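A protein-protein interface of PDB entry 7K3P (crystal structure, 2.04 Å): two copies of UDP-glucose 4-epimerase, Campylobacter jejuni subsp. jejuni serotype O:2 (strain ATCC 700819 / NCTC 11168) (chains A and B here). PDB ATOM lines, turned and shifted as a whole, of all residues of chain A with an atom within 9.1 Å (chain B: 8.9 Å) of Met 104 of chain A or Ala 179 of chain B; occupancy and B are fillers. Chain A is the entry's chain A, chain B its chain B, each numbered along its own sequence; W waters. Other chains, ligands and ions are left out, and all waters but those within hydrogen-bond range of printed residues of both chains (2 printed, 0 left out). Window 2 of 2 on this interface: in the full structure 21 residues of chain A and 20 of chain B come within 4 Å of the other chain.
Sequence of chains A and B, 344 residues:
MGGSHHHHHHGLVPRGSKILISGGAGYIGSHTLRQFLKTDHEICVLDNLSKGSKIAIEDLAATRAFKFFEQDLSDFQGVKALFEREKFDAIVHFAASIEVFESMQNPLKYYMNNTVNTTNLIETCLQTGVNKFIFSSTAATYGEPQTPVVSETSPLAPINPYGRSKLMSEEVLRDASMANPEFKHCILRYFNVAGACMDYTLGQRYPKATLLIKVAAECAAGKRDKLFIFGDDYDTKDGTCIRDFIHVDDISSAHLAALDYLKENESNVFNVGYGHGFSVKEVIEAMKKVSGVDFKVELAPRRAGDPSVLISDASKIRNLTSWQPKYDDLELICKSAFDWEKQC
Water W1 lies within hydrogen-bond range of O of Gln 105 of chain A (2.9 Å) and O of Ala 179 of chain B (3.1 Å). Water W2 bridges NE of Arg 164 of chain A (3.2 Å) and OD1 of Asp 175 of chain B (3.3 Å).
Met 104 of chain A touches Ala 179 of chain B. Gln 105 of chain A touches Ala 179 of chain B (O to CB, 3.8 Å). Pro 107 of chain A touches Asp 175 of chain B. CD of Pro 107 of chain A touches CB of Ala 179 of chain B, 3.5 Å away. CD2 of Leu 108 of chain A touches CD1 of Leu 126 of chain B, 3.5 Å away. CD1 of Leu 108 of chain A touches CG1 of Val 172 of chain B, 3.7 Å away. CB of Ala 176 of chain B touches CD2 of Leu 108 of chain A, 3.9 Å away. CG of Tyr 111 of chain A touches CG2 of Val 172 of chain B, 3.8 Å away. Pro 161 of chain A touches Asp 175 of chain B.
No residue of chain B comes within 4 Å of Ser 103 of chain A. Of chain B, only Ala 179 comes within 4 Å of Met 104 of chain A. Of the printed residues of chain B, Tyr 111 of chain A touches Val 172 and Asp 175. Gly 163 of chain A touches none of the printed residues of chain B. Of the printed residues of chain A, Leu 126 of chain B touches Leu 108 (3.5 Å). Ala 179 of chain B touches just these residues of chain A: Met 104 (3.5 Å), Gln 105 (3.8 Å) and Pro 107 (3.5 Å). The nearest residue of chain B that does not touch Met 104 of chain A is Asp 175 of chain B (5.7 Å). The nearest residue of chain A that does not touch Ala 179 of chain B is Asn 106 of chain A (5.0 Å). The nearest printed residue of chain B that does not touch Gln 105 of chain A is Asn 180 of chain B (5.4 Å).
The side-chain hydroxyl (OH) of Tyr 111 of chain A lies close to the guanidinium group (NE) of Arg 164 of chain A (3.4 Å). ND2 of Asn 180 of chain B is in hydrogen-bond range of O of Ala 176 of chain B, 3.1 Å away.
The side-chain carboxylate (OD2) of Asp 175 of chain B is in hydrogen-bond range of the side-chain hydroxyl (OH) of Tyr 111 of chain A (2.6 Å). OD2 of Asp 175 of chain B is in salt-bridge range of NE of Arg 164 of chain A.
Of the 22 printed residues of chain A, 7 touch a printed residue of chain B. Hydrophobic or aromatic side chains of chain A within 4 Å of the printed part of chain B: Pro 107, Leu 108, Tyr 111 and Pro 161. Along chain A the printed residues that touch a printed residue of chain B span positions 104 to 164. Of the 13 printed residues of chain B, 5 touch a printed residue of chain A. Printed residues of chain B that touch a printed residue of chain A: Leu 126, Val 172, Asp 175, Ala 176 and Ala 179.
No position is printed for both chains. Of the 11 pairs that touch across the chains among the printed residues, none has its exchanged pair printed and touching as well.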
ATOM      1  N   GLU A  99     -27.921 -22.141 -15.016  1.00  0.00           N
ATOM      2  CA  GLU A  99     -27.573 -22.667 -16.344  1.00  0.00           C
ATOM      3  C   GLU A  99     -26.344 -21.982 -16.947  1.00  0.00           C
ATOM      4  O   GLU A  99     -26.411 -20.811 -17.363  1.00  0.00           O
ATOM      5  CB  GLU A  99     -28.762 -22.524 -17.311  1.00  0.00           C
ATOM      6  CG  GLU A  99     -30.104 -22.927 -16.699  1.00  0.00           C
ATOM      7  CD  GLU A  99     -30.943 -23.808 -17.603  1.00  0.00           C
ATOM      8  OE1 GLU A  99     -30.369 -24.530 -18.446  1.00  0.00           O
ATOM      9  OE2 GLU A  99     -32.185 -23.783 -17.466  1.00  0.00           O
ATOM     10  N   VAL A 100     -25.239 -22.723 -16.997  1.00  0.00           N
ATOM     11  CA  VAL A 100     -23.994 -22.248 -17.597  1.00  0.00           C
ATOM     12  C   VAL A 100     -24.231 -21.604 -18.966  1.00  0.00           C
ATOM     13  O   VAL A 100     -23.832 -20.463 -19.200  1.00  0.00           O
ATOM     14  CB  VAL A 100     -22.957 -23.387 -17.705  1.00  0.00           C
ATOM     15  CG1 VAL A 100     -21.873 -23.061 -18.746  1.00  0.00           C
ATOM     16  CG2 VAL A 100     -22.323 -23.672 -16.340  1.00  0.00           C
ATOM     17  N   PHE A 101     -24.910 -22.321 -19.858  1.00  0.00           N
ATOM     18  CA  PHE A 101     -25.133 -21.809 -21.209  1.00  0.00           C
ATOM     19  C   PHE A 101     -25.848 -20.456 -21.214  1.00  0.00           C
ATOM     20  O   PHE A 101     -25.487 -19.558 -21.981  1.00  0.00           O
ATOM     21  CB  PHE A 101     -25.894 -22.822 -22.072  1.00  0.00           C
ATOM     22  CG  PHE A 101     -25.923 -22.461 -23.537  1.00  0.00           C
ATOM     23  CD1 PHE A 101     -26.823 -21.511 -24.021  1.00  0.00           C
ATOM     24  CD2 PHE A 101     -25.042 -23.061 -24.428  1.00  0.00           C
ATOM     25  CE1 PHE A 101     -26.845 -21.172 -25.372  1.00  0.00           C
ATOM     26  CE2 PHE A 101     -25.063 -22.731 -25.779  1.00  0.00           C
ATOM     27  CZ  PHE A 101     -25.964 -21.782 -26.250  1.00  0.00           C
ATOM     28  N   GLU A 102     -26.863 -20.306 -20.363  1.00  0.00           N
ATOM     29  CA  GLU A 102     -27.591 -19.044 -20.298  1.00  0.00           C
ATOM     30  C   GLU A 102     -26.690 -17.935 -19.762  1.00  0.00           C
ATOM     31  O   GLU A 102     -26.807 -16.784 -20.180  1.00  0.00           O
ATOM     32  CB  GLU A 102     -28.852 -19.168 -19.429  1.00  0.00           C
ATOM     33  CG  GLU A 102     -29.736 -17.915 -19.436  1.00  0.00           C
ATOM     34  CD  GLU A 102     -30.810 -17.928 -18.340  1.00  0.00           C
ATOM     35  OE1 GLU A 102     -30.667 -18.687 -17.348  1.00  0.00           O
ATOM     36  OE2 GLU A 102     -31.792 -17.169 -18.477  1.00  0.00           O
ATOM     37  N   SER A 103     -25.788 -18.278 -18.843  1.00  0.00           N
ATOM     38  CA  SER A 103     -24.945 -17.263 -18.198  1.00  0.00           C
ATOM     39  C   SER A 103     -23.938 -16.666 -19.175  1.00  0.00           C
ATOM     40  O   SER A 103     -23.557 -15.495 -19.053  1.00  0.00           O
ATOM     41  CB  SER A 103     -24.211 -17.833 -16.973  1.00  0.00           C
ATOM     42  OG  SER A 103     -23.125 -18.675 -17.346  1.00  0.00           O
ATOM     43  N   MET A 104     -23.506 -17.475 -20.140  1.00  0.00           N
ATOM     44  CA  MET A 104     -22.607 -16.999 -21.188  1.00  0.00           C
ATOM     45  C   MET A 104     -23.305 -15.966 -22.055  1.00  0.00           C
ATOM     46  O   MET A 104     -22.698 -14.978 -22.471  1.00  0.00           O
ATOM     47  CB  MET A 104     -22.096 -18.175 -22.032  1.00  0.00           C
ATOM     48  CG  MET A 104     -21.205 -19.133 -21.242  1.00  0.00           C
ATOM     49  SD  MET A 104     -20.839 -20.731 -22.034  1.00  0.00           S
ATOM     50  CE  MET A 104     -19.830 -20.212 -23.425  1.00  0.00           C
ATOM     51  N   GLN A 105     -24.597 -16.172 -22.298  1.00  0.00           N
ATOM     52  CA  GLN A 105     -25.364 -15.230 -23.111  1.00  0.00           C
ATOM     53  C   GLN A 105     -25.874 -14.021 -22.330  1.00  0.00           C
ATOM     54  O   GLN A 105     -26.019 -12.938 -22.890  1.00  0.00           O
ATOM     55  CB  GLN A 105     -26.529 -15.939 -23.807  1.00  0.00           C
ATOM     56  CG  GLN A 105     -26.086 -16.699 -25.048  1.00  0.00           C
ATOM     57  CD  GLN A 105     -27.055 -17.796 -25.440  1.00  0.00           C
ATOM     58  OE1 GLN A 105     -28.022 -18.079 -24.724  1.00  0.00           O
ATOM     59  NE2 GLN A 105     -26.800 -18.423 -26.586  1.00  0.00           N
ATOM     60  N   ASN A 106     -26.136 -14.210 -21.038  1.00  0.00           N
ATOM     61  CA  ASN A 106     -26.757 -13.170 -20.235  1.00  0.00           C
ATOM     62  C   ASN A 106     -26.064 -13.108 -18.880  1.00  0.00           C
ATOM     63  O   ASN A 106     -26.657 -13.453 -17.858  1.00  0.00           O
ATOM     64  CB  ASN A 106     -28.254 -13.490 -20.059  1.00  0.00           C
ATOM     65  CG  ASN A 106     -29.039 -12.348 -19.436  1.00  0.00           C
ATOM     66  OD1 ASN A 106     -28.470 -11.354 -18.970  1.00  0.00           O
ATOM     67  ND2 ASN A 106     -30.363 -12.487 -19.425  1.00  0.00           N
ATOM     68  N   PRO A 107     -24.796 -12.679 -18.868  1.00  0.00           N
ATOM     69  CA  PRO A 107     -24.044 -12.674 -17.610  1.00  0.00           C
ATOM     70  C   PRO A 107     -24.685 -11.808 -16.532  1.00  0.00           C
ATOM     71  O   PRO A 107     -24.631 -12.207 -15.372  1.00  0.00           O
ATOM     72  CB  PRO A 107     -22.669 -12.104 -18.008  1.00  0.00           C
ATOM     73  CG  PRO A 107     -22.905 -11.413 -19.367  1.00  0.00           C
ATOM     74  CD  PRO A 107     -23.963 -12.271 -20.015  1.00  0.00           C
ATOM     75  N   LEU A 108     -25.264 -10.659 -16.882  1.00  0.00           N
ATOM     76  CA  LEU A 108     -25.768  -9.761 -15.842  1.00  0.00           C
ATOM     77  C   LEU A 108     -26.936 -10.372 -15.046  1.00  0.00           C
ATOM     78  O   LEU A 108     -27.106 -10.092 -13.853  1.00  0.00           O
ATOM     79  CB  LEU A 108     -26.079  -8.357 -16.400  1.00  0.00           C
ATOM     80  CG  LEU A 108     -24.895  -7.364 -16.401  1.00  0.00           C
ATOM     81  CD1 LEU A 108     -24.425  -7.116 -14.976  1.00  0.00           C
ATOM     82  CD2 LEU A 108     -23.710  -7.823 -17.259  1.00  0.00           C
ATOM     83  N   LYS A 109     -27.716 -11.235 -15.684  1.00  0.00           N
ATOM     84  CA  LYS A 109     -28.780 -11.948 -14.972  1.00  0.00           C
ATOM     85  C   LYS A 109     -28.189 -12.829 -13.864  1.00  0.00           C
ATOM     86  O   LYS A 109     -28.759 -12.959 -12.771  1.00  0.00           O
ATOM     87  CB  LYS A 109     -29.596 -12.803 -15.952  1.00  0.00           C
ATOM     88  CG  LYS A 109     -30.517 -13.820 -15.293  1.00  0.00           C
ATOM     89  CD  LYS A 109     -31.390 -14.558 -16.327  1.00  0.00           C
ATOM     90  CE  LYS A 109     -32.357 -15.516 -15.642  1.00  0.00           C
ATOM     91  NZ  LYS A 109     -33.275 -16.229 -16.592  1.00  0.00           N
ATOM     92  N   TYR A 110     -27.041 -13.430 -14.151  1.00  0.00           N
ATOM     93  CA  TYR A 110     -26.384 -14.312 -13.188  1.00  0.00           C
ATOM     94  C   TYR A 110     -25.735 -13.526 -12.046  1.00  0.00           C
ATOM     95  O   TYR A 110     -25.939 -13.843 -10.876  1.00  0.00           O
ATOM     96  CB  TYR A 110     -25.438 -15.293 -13.904  1.00  0.00           C
ATOM     97  CG  TYR A 110     -26.274 -16.409 -14.475  1.00  0.00           C
ATOM     98  CD1 TYR A 110     -27.148 -16.173 -15.534  1.00  0.00           C
ATOM     99  CD2 TYR A 110     -26.274 -17.669 -13.892  1.00  0.00           C
ATOM    100  CE1 TYR A 110     -27.971 -17.177 -16.017  1.00  0.00           C
ATOM    101  CE2 TYR A 110     -27.081 -18.672 -14.373  1.00  0.00           C
ATOM    102  CZ  TYR A 110     -27.928 -18.423 -15.431  1.00  0.00           C
ATOM    103  OH  TYR A 110     -28.741 -19.431 -15.890  1.00  0.00           O
ATOM    104  N   TYR A 111     -25.003 -12.471 -12.374  1.00  0.00           N
ATOM    105  CA  TYR A 111     -24.453 -11.624 -11.332  1.00  0.00           C
ATOM    106  C   TYR A 111     -25.521 -10.949 -10.460  1.00  0.00           C
ATOM    107  O   TYR A 111     -25.287 -10.730  -9.270  1.00  0.00           O
ATOM    108  CB  TYR A 111     -23.490 -10.589 -11.916  1.00  0.00           C
ATOM    109  CG  TYR A 111     -22.214 -11.214 -12.438  1.00  0.00           C
ATOM    110  CD1 TYR A 111     -21.327 -11.864 -11.569  1.00  0.00           C
ATOM    111  CD2 TYR A 111     -21.893 -11.163 -13.791  1.00  0.00           C
ATOM    112  CE1 TYR A 111     -20.148 -12.444 -12.039  1.00  0.00           C
ATOM    113  CE2 TYR A 111     -20.706 -11.746 -14.283  1.00  0.00           C
ATOM    114  CZ  TYR A 111     -19.850 -12.383 -13.404  1.00  0.00           C
ATOM    115  OH  TYR A 111     -18.689 -12.945 -13.872  1.00  0.00           O
ATOM    116  N   ILE A 159     -14.779 -20.604 -15.492  1.00  0.00           N
ATOM    117  CA  ILE A 159     -14.606 -20.213 -16.884  1.00  0.00           C
ATOM    118  C   ILE A 159     -15.906 -19.701 -17.501  1.00  0.00           C
ATOM    119  O   ILE A 159     -15.985 -19.505 -18.710  1.00  0.00           O
ATOM    120  CB  ILE A 159     -14.077 -21.385 -17.739  1.00  0.00           C
ATOM    121  CG1 ILE A 159     -15.073 -22.547 -17.724  1.00  0.00           C
ATOM    122  CG2 ILE A 159     -12.722 -21.841 -17.225  1.00  0.00           C
ATOM    123  CD1 ILE A 159     -14.689 -23.702 -18.655  1.00  0.00           C
ATOM    124  N   ASN A 160     -16.930 -19.498 -16.679  1.00  0.00           N
ATOM    125  CA  ASN A 160     -18.153 -18.878 -17.171  1.00  0.00           C
ATOM    126  C   ASN A 160     -18.775 -18.004 -16.091  1.00  0.00           C
ATOM    127  O   ASN A 160     -18.383 -18.086 -14.930  1.00  0.00           O
ATOM    128  CB  ASN A 160     -19.140 -19.933 -17.665  1.00  0.00           C
ATOM    129  CG  ASN A 160     -19.404 -20.999 -16.630  1.00  0.00           C
ATOM    130  OD1 ASN A 160     -20.053 -20.736 -15.607  1.00  0.00           O
ATOM    131  ND2 ASN A 160     -18.901 -22.215 -16.882  1.00  0.00           N
ATOM    132  N   PRO A 161     -19.723 -17.134 -16.478  1.00  0.00           N
ATOM    133  CA  PRO A 161     -20.272 -16.200 -15.490  1.00  0.00           C
ATOM    134  C   PRO A 161     -21.047 -16.915 -14.379  1.00  0.00           C
ATOM    135  O   PRO A 161     -21.047 -16.413 -13.250  1.00  0.00           O
ATOM    136  CB  PRO A 161     -21.195 -15.303 -16.328  1.00  0.00           C
ATOM    137  CG  PRO A 161     -20.619 -15.406 -17.768  1.00  0.00           C
ATOM    138  CD  PRO A 161     -20.188 -16.849 -17.851  1.00  0.00           C
ATOM    139  N   TYR A 162     -21.692 -18.045 -14.674  1.00  0.00           N
ATOM    140  CA  TYR A 162     -22.354 -18.797 -13.613  1.00  0.00           C
ATOM    141  C   TYR A 162     -21.334 -19.194 -12.549  1.00  0.00           C
ATOM    142  O   TYR A 162     -21.525 -18.924 -11.361  1.00  0.00           O
ATOM    143  CB  TYR A 162     -23.067 -20.040 -14.155  1.00  0.00           C
ATOM    144  CG  TYR A 162     -23.523 -21.016 -13.066  1.00  0.00           C
ATOM    145  CD1 TYR A 162     -24.538 -20.674 -12.170  1.00  0.00           C
ATOM    146  CD2 TYR A 162     -22.932 -22.272 -12.936  1.00  0.00           C
ATOM    147  CE1 TYR A 162     -24.953 -21.554 -11.178  1.00  0.00           C
ATOM    148  CE2 TYR A 162     -23.343 -23.161 -11.949  1.00  0.00           C
ATOM    149  CZ  TYR A 162     -24.356 -22.798 -11.081  1.00  0.00           C
ATOM    150  OH  TYR A 162     -24.759 -23.690 -10.122  1.00  0.00           O
ATOM    151  N   GLY A 163     -20.239 -19.823 -12.975  1.00  0.00           N
ATOM    152  CA  GLY A 163     -19.202 -20.234 -12.039  1.00  0.00           C
ATOM    153  C   GLY A 163     -18.598 -19.073 -11.263  1.00  0.00           C
ATOM    154  O   GLY A 163     -18.363 -19.178 -10.048  1.00  0.00           O
ATOM    155  N   ARG A 164     -18.331 -17.970 -11.960  1.00  0.00           N
ATOM    156  CA  ARG A 164     -17.811 -16.767 -11.317  1.00  0.00           C
ATOM    157  C   ARG A 164     -18.803 -16.183 -10.319  1.00  0.00           C
ATOM    158  O   ARG A 164     -18.402 -15.702  -9.256  1.00  0.00           O
ATOM    159  CB  ARG A 164     -17.435 -15.694 -12.358  1.00  0.00           C
ATOM    160  CG  ARG A 164     -16.144 -15.995 -13.110  1.00  0.00           C
ATOM    161  CD  ARG A 164     -15.719 -14.870 -14.034  1.00  0.00           C
ATOM    162  NE  ARG A 164     -16.363 -14.961 -15.340  1.00  0.00           N
ATOM    163  CZ  ARG A 164     -15.929 -15.740 -16.332  1.00  0.00           C
ATOM    164  NH1 ARG A 164     -14.859 -16.499 -16.144  1.00  0.00           N
ATOM    165  NH2 ARG A 164     -16.566 -15.770 -17.506  1.00  0.00           N
ATOM    166  N   TYR A 200     -31.699 -24.955 -21.168  1.00  0.00           N
ATOM    167  CA  TYR A 200     -30.695 -24.704 -22.202  1.00  0.00           C
ATOM    168  C   TYR A 200     -29.914 -25.933 -22.661  1.00  0.00           C
ATOM    169  O   TYR A 200     -29.053 -25.837 -23.533  1.00  0.00           O
ATOM    170  CB  TYR A 200     -29.751 -23.577 -21.768  1.00  0.00           C
ATOM    171  CG  TYR A 200     -30.449 -22.243 -21.760  1.00  0.00           C
ATOM    172  CD1 TYR A 200     -31.236 -21.853 -20.682  1.00  0.00           C
ATOM    173  CD2 TYR A 200     -30.363 -21.395 -22.856  1.00  0.00           C
ATOM    174  CE1 TYR A 200     -31.899 -20.637 -20.691  1.00  0.00           C
ATOM    175  CE2 TYR A 200     -31.017 -20.185 -22.873  1.00  0.00           C
ATOM    176  CZ  TYR A 200     -31.780 -19.807 -21.794  1.00  0.00           C
ATOM    177  OH  TYR A 200     -32.431 -18.597 -21.823  1.00  0.00           O
ATOM    178  N   GLN A 204     -28.450 -27.854 -27.044  1.00  0.00           N
ATOM    179  CA  GLN A 204     -27.034 -28.142 -27.302  1.00  0.00           C
ATOM    180  C   GLN A 204     -26.913 -29.522 -27.946  1.00  0.00           C
ATOM    181  O   GLN A 204     -27.344 -30.529 -27.365  1.00  0.00           O
ATOM    182  CB  GLN A 204     -26.220 -28.119 -26.004  1.00  0.00           C
ATOM    183  CG  GLN A 204     -26.160 -26.773 -25.279  1.00  0.00           C
ATOM    184  CD  GLN A 204     -25.461 -26.873 -23.919  1.00  0.00           C
ATOM    185  OE1 GLN A 204     -24.303 -27.291 -23.830  1.00  0.00           O
ATOM    186  NE2 GLN A 204     -26.176 -26.506 -22.856  1.00  0.00           N
ATOM    187  N   LYS A 208     -21.364 -31.157 -22.839  1.00  0.00           N
ATOM    188  CA  LYS A 208     -20.254 -31.705 -22.064  1.00  0.00           C
ATOM    189  C   LYS A 208     -20.679 -32.989 -21.367  1.00  0.00           C
ATOM    190  O   LYS A 208     -21.875 -33.204 -21.125  1.00  0.00           O
ATOM    191  CB  LYS A 208     -19.772 -30.690 -21.024  1.00  0.00           C
ATOM    192  CG  LYS A 208     -19.045 -29.476 -21.616  1.00  0.00           C
ATOM    193  CD  LYS A 208     -17.644 -29.834 -22.110  1.00  0.00           C
ATOM    194  CE  LYS A 208     -16.949 -28.626 -22.743  1.00  0.00           C
ATOM    195  NZ  LYS A 208     -15.538 -28.930 -23.142  1.00  0.00           N
ATOM    196  N   LEU B 126     -26.176  -1.611 -20.156  1.00  0.00           N
ATOM    197  CA  LEU B 126     -26.541  -2.534 -21.225  1.00  0.00           C
ATOM    198  C   LEU B 126     -27.991  -2.360 -21.680  1.00  0.00           C
ATOM    199  O   LEU B 126     -28.278  -2.438 -22.877  1.00  0.00           O
ATOM    200  CB  LEU B 126     -26.299  -3.980 -20.787  1.00  0.00           C
ATOM    201  CG  LEU B 126     -24.825  -4.333 -20.618  1.00  0.00           C
ATOM    202  CD1 LEU B 126     -24.669  -5.690 -19.925  1.00  0.00           C
ATOM    203  CD2 LEU B 126     -24.118  -4.335 -21.988  1.00  0.00           C
ATOM    204  N   VAL B 172     -17.217  -8.584 -13.881  1.00  0.00           N
ATOM    205  CA  VAL B 172     -18.531  -8.347 -14.473  1.00  0.00           C
ATOM    206  C   VAL B 172     -18.394  -7.552 -15.791  1.00  0.00           C
ATOM    207  O   VAL B 172     -19.025  -7.889 -16.800  1.00  0.00           O
ATOM    208  CB  VAL B 172     -19.469  -7.616 -13.505  1.00  0.00           C
ATOM    209  CG1 VAL B 172     -20.843  -7.393 -14.149  1.00  0.00           C
ATOM    210  CG2 VAL B 172     -19.625  -8.428 -12.202  1.00  0.00           C
ATOM    211  N   LEU B 173     -17.581  -6.496 -15.785  1.00  0.00           N
ATOM    212  CA  LEU B 173     -17.354  -5.715 -17.012  1.00  0.00           C
ATOM    213  C   LEU B 173     -16.802  -6.581 -18.159  1.00  0.00           C
ATOM    214  O   LEU B 173     -17.261  -6.485 -19.295  1.00  0.00           O
ATOM    215  CB  LEU B 173     -16.408  -4.542 -16.751  1.00  0.00           C
ATOM    216  CG  LEU B 173     -16.991  -3.356 -15.991  1.00  0.00           C
ATOM    217  CD1 LEU B 173     -15.892  -2.376 -15.650  1.00  0.00           C
ATOM    218  CD2 LEU B 173     -18.069  -2.670 -16.828  1.00  0.00           C
ATOM    219  N   ARG B 174     -15.810  -7.413 -17.857  1.00  0.00           N
ATOM    220  CA  ARG B 174     -15.249  -8.333 -18.845  1.00  0.00           C
ATOM    221  C   ARG B 174     -16.314  -9.236 -19.440  1.00  0.00           C
ATOM    222  O   ARG B 174     -16.386  -9.390 -20.662  1.00  0.00           O
ATOM    223  CB  ARG B 174     -14.127  -9.167 -18.232  1.00  0.00           C
ATOM    224  CG  ARG B 174     -12.739  -8.596 -18.485  1.00  0.00           C
ATOM    225  CD  ARG B 174     -11.710  -9.016 -17.434  1.00  0.00           C
ATOM    226  NE  ARG B 174     -11.027  -7.798 -17.029  1.00  0.00           N
ATOM    227  CZ  ARG B 174     -10.511  -7.546 -15.839  1.00  0.00           C
ATOM    228  NH1 ARG B 174     -10.538  -8.449 -14.860  1.00  0.00           N
ATOM    229  NH2 ARG B 174      -9.949  -6.369 -15.648  1.00  0.00           N
ATOM    230  N   ASP B 175     -17.148  -9.826 -18.587  1.00  0.00           N
ATOM    231  CA  ASP B 175     -18.235 -10.675 -19.070  1.00  0.00           C
ATOM    232  C   ASP B 175     -19.286  -9.877 -19.847  1.00  0.00           C
ATOM    233  O   ASP B 175     -19.836 -10.369 -20.830  1.00  0.00           O
ATOM    234  CB  ASP B 175     -18.881 -11.464 -17.921  1.00  0.00           C
ATOM    235  CG  ASP B 175     -18.063 -12.668 -17.523  1.00  0.00           C
ATOM    236  OD1 ASP B 175     -17.234 -13.100 -18.338  1.00  0.00           O
ATOM    237  OD2 ASP B 175     -18.243 -13.201 -16.409  1.00  0.00           O
ATOM    238  N   ALA B 176     -19.555  -8.651 -19.416  1.00  0.00           N
ATOM    239  CA  ALA B 176     -20.528  -7.812 -20.116  1.00  0.00           C
ATOM    240  C   ALA B 176     -20.067  -7.569 -21.562  1.00  0.00           C
ATOM    241  O   ALA B 176     -20.845  -7.708 -22.507  1.00  0.00           O
ATOM    242  CB  ALA B 176     -20.710  -6.479 -19.391  1.00  0.00           C
ATOM    243  N   SER B 177     -18.802  -7.196 -21.726  1.00  0.00           N
ATOM    244  CA  SER B 177     -18.279  -6.913 -23.064  1.00  0.00           C
ATOM    245  C   SER B 177     -18.156  -8.171 -23.920  1.00  0.00           C
ATOM    246  O   SER B 177     -18.315  -8.107 -25.137  1.00  0.00           O
ATOM    247  CB  SER B 177     -16.940  -6.186 -22.986  1.00  0.00           C
ATOM    248  OG  SER B 177     -17.108  -4.921 -22.374  1.00  0.00           O
ATOM    249  N   MET B 178     -17.888  -9.314 -23.292  1.00  0.00           N
ATOM    250  CA  MET B 178     -17.835 -10.572 -24.034  1.00  0.00           C
ATOM    251  C   MET B 178     -19.197 -10.939 -24.607  1.00  0.00           C
ATOM    252  O   MET B 178     -19.305 -11.346 -25.761  1.00  0.00           O
ATOM    253  CB  MET B 178     -17.303 -11.713 -23.162  1.00  0.00           C
ATOM    254  CG  MET B 178     -15.803 -11.639 -22.883  1.00  0.00           C
ATOM    255  SD  MET B 178     -14.743 -11.744 -24.359  1.00  0.00           S
ATOM    256  CE  MET B 178     -15.113 -13.416 -24.903  1.00  0.00           C
ATOM    257  N   ALA B 179     -20.243 -10.798 -23.807  1.00  0.00           N
ATOM    258  CA  ALA B 179     -21.576 -11.147 -24.282  1.00  0.00           C
ATOM    259  C   ALA B 179     -22.223 -10.015 -25.104  1.00  0.00           C
ATOM    260  O   ALA B 179     -23.252 -10.226 -25.752  1.00  0.00           O
ATOM    261  CB  ALA B 179     -22.471 -11.560 -23.107  1.00  0.00           C
ATOM    262  N   ASN B 180     -21.614  -8.826 -25.069  1.00  0.00           N
ATOM    263  CA  ASN B 180     -22.147  -7.631 -25.743  1.00  0.00           C
ATOM    264  C   ASN B 180     -21.039  -6.795 -26.397  1.00  0.00           C
ATOM    265  O   ASN B 180     -20.691  -5.724 -25.895  1.00  0.00           O
ATOM    266  CB  ASN B 180     -22.912  -6.733 -24.762  1.00  0.00           C
ATOM    267  CG  ASN B 180     -24.088  -7.434 -24.124  1.00  0.00           C
ATOM    268  OD1 ASN B 180     -25.184  -7.473 -24.690  1.00  0.00           O
ATOM    269  ND2 ASN B 180     -23.869  -7.991 -22.929  1.00  0.00           N
ATOM    270  N   PRO B 181     -20.509  -7.268 -27.540  1.00  0.00           N
ATOM    271  CA  PRO B 181     -19.392  -6.663 -28.284  1.00  0.00           C
ATOM    272  C   PRO B 181     -19.503  -5.150 -28.470  1.00  0.00           C
ATOM    273  O   PRO B 181     -18.477  -4.483 -28.503  1.00  0.00           O
ATOM    274  CB  PRO B 181     -19.435  -7.382 -29.646  1.00  0.00           C
ATOM    275  CG  PRO B 181     -20.743  -8.146 -29.664  1.00  0.00           C
ATOM    276  CD  PRO B 181     -21.056  -8.442 -28.238  1.00  0.00           C
ATOM    277  N   GLU B 182     -20.716  -4.625 -28.577  1.00  0.00           N
ATOM    278  CA  GLU B 182     -20.940  -3.176 -28.631  1.00  0.00           C
ATOM    279  C   GLU B 182     -20.591  -2.444 -27.316  1.00  0.00           C
ATOM    280  O   GLU B 182     -20.290  -1.243 -27.306  1.00  0.00           O
ATOM    281  CB  GLU B 182     -22.393  -2.876 -29.036  1.00  0.00           C
ATOM    282  CG  GLU B 182     -23.469  -3.346 -28.036  1.00  0.00           C
ATOM    283  CD  GLU B 182     -23.673  -4.862 -28.028  1.00  0.00           C
ATOM    284  OE1 GLU B 182     -22.738  -5.593 -28.406  1.00  0.00           O
ATOM    285  OE2 GLU B 182     -24.774  -5.327 -27.647  1.00  0.00           O
ATOM    286  N   PHE B 183     -20.625  -3.164 -26.201  1.00  0.00           N
ATOM    287  CA  PHE B 183     -20.345  -2.543 -24.909  1.00  0.00           C
ATOM    288  C   PHE B 183     -18.832  -2.515 -24.640  1.00  0.00           C
ATOM    289  O   PHE B 183     -18.201  -3.559 -24.506  1.00  0.00           O
ATOM    290  CB  PHE B 183     -21.100  -3.292 -23.802  1.00  0.00           C
ATOM    291  CG  PHE B 183     -20.837  -2.765 -22.429  1.00  0.00           C
ATOM    292  CD1 PHE B 183     -21.444  -1.590 -21.993  1.00  0.00           C
ATOM    293  CD2 PHE B 183     -19.991  -3.444 -21.569  1.00  0.00           C
ATOM    294  CE1 PHE B 183     -21.204  -1.095 -20.716  1.00  0.00           C
ATOM    295  CE2 PHE B 183     -19.748  -2.966 -20.291  1.00  0.00           C
ATOM    296  CZ  PHE B 183     -20.353  -1.787 -19.862  1.00  0.00           C
HETATM  297  O   HOH W   1     -25.374 -12.522 -25.654  1.00  0.00           O
HETATM  298  O   HOH W   2     -14.823 -12.255 -16.258  1.00  0.00           O
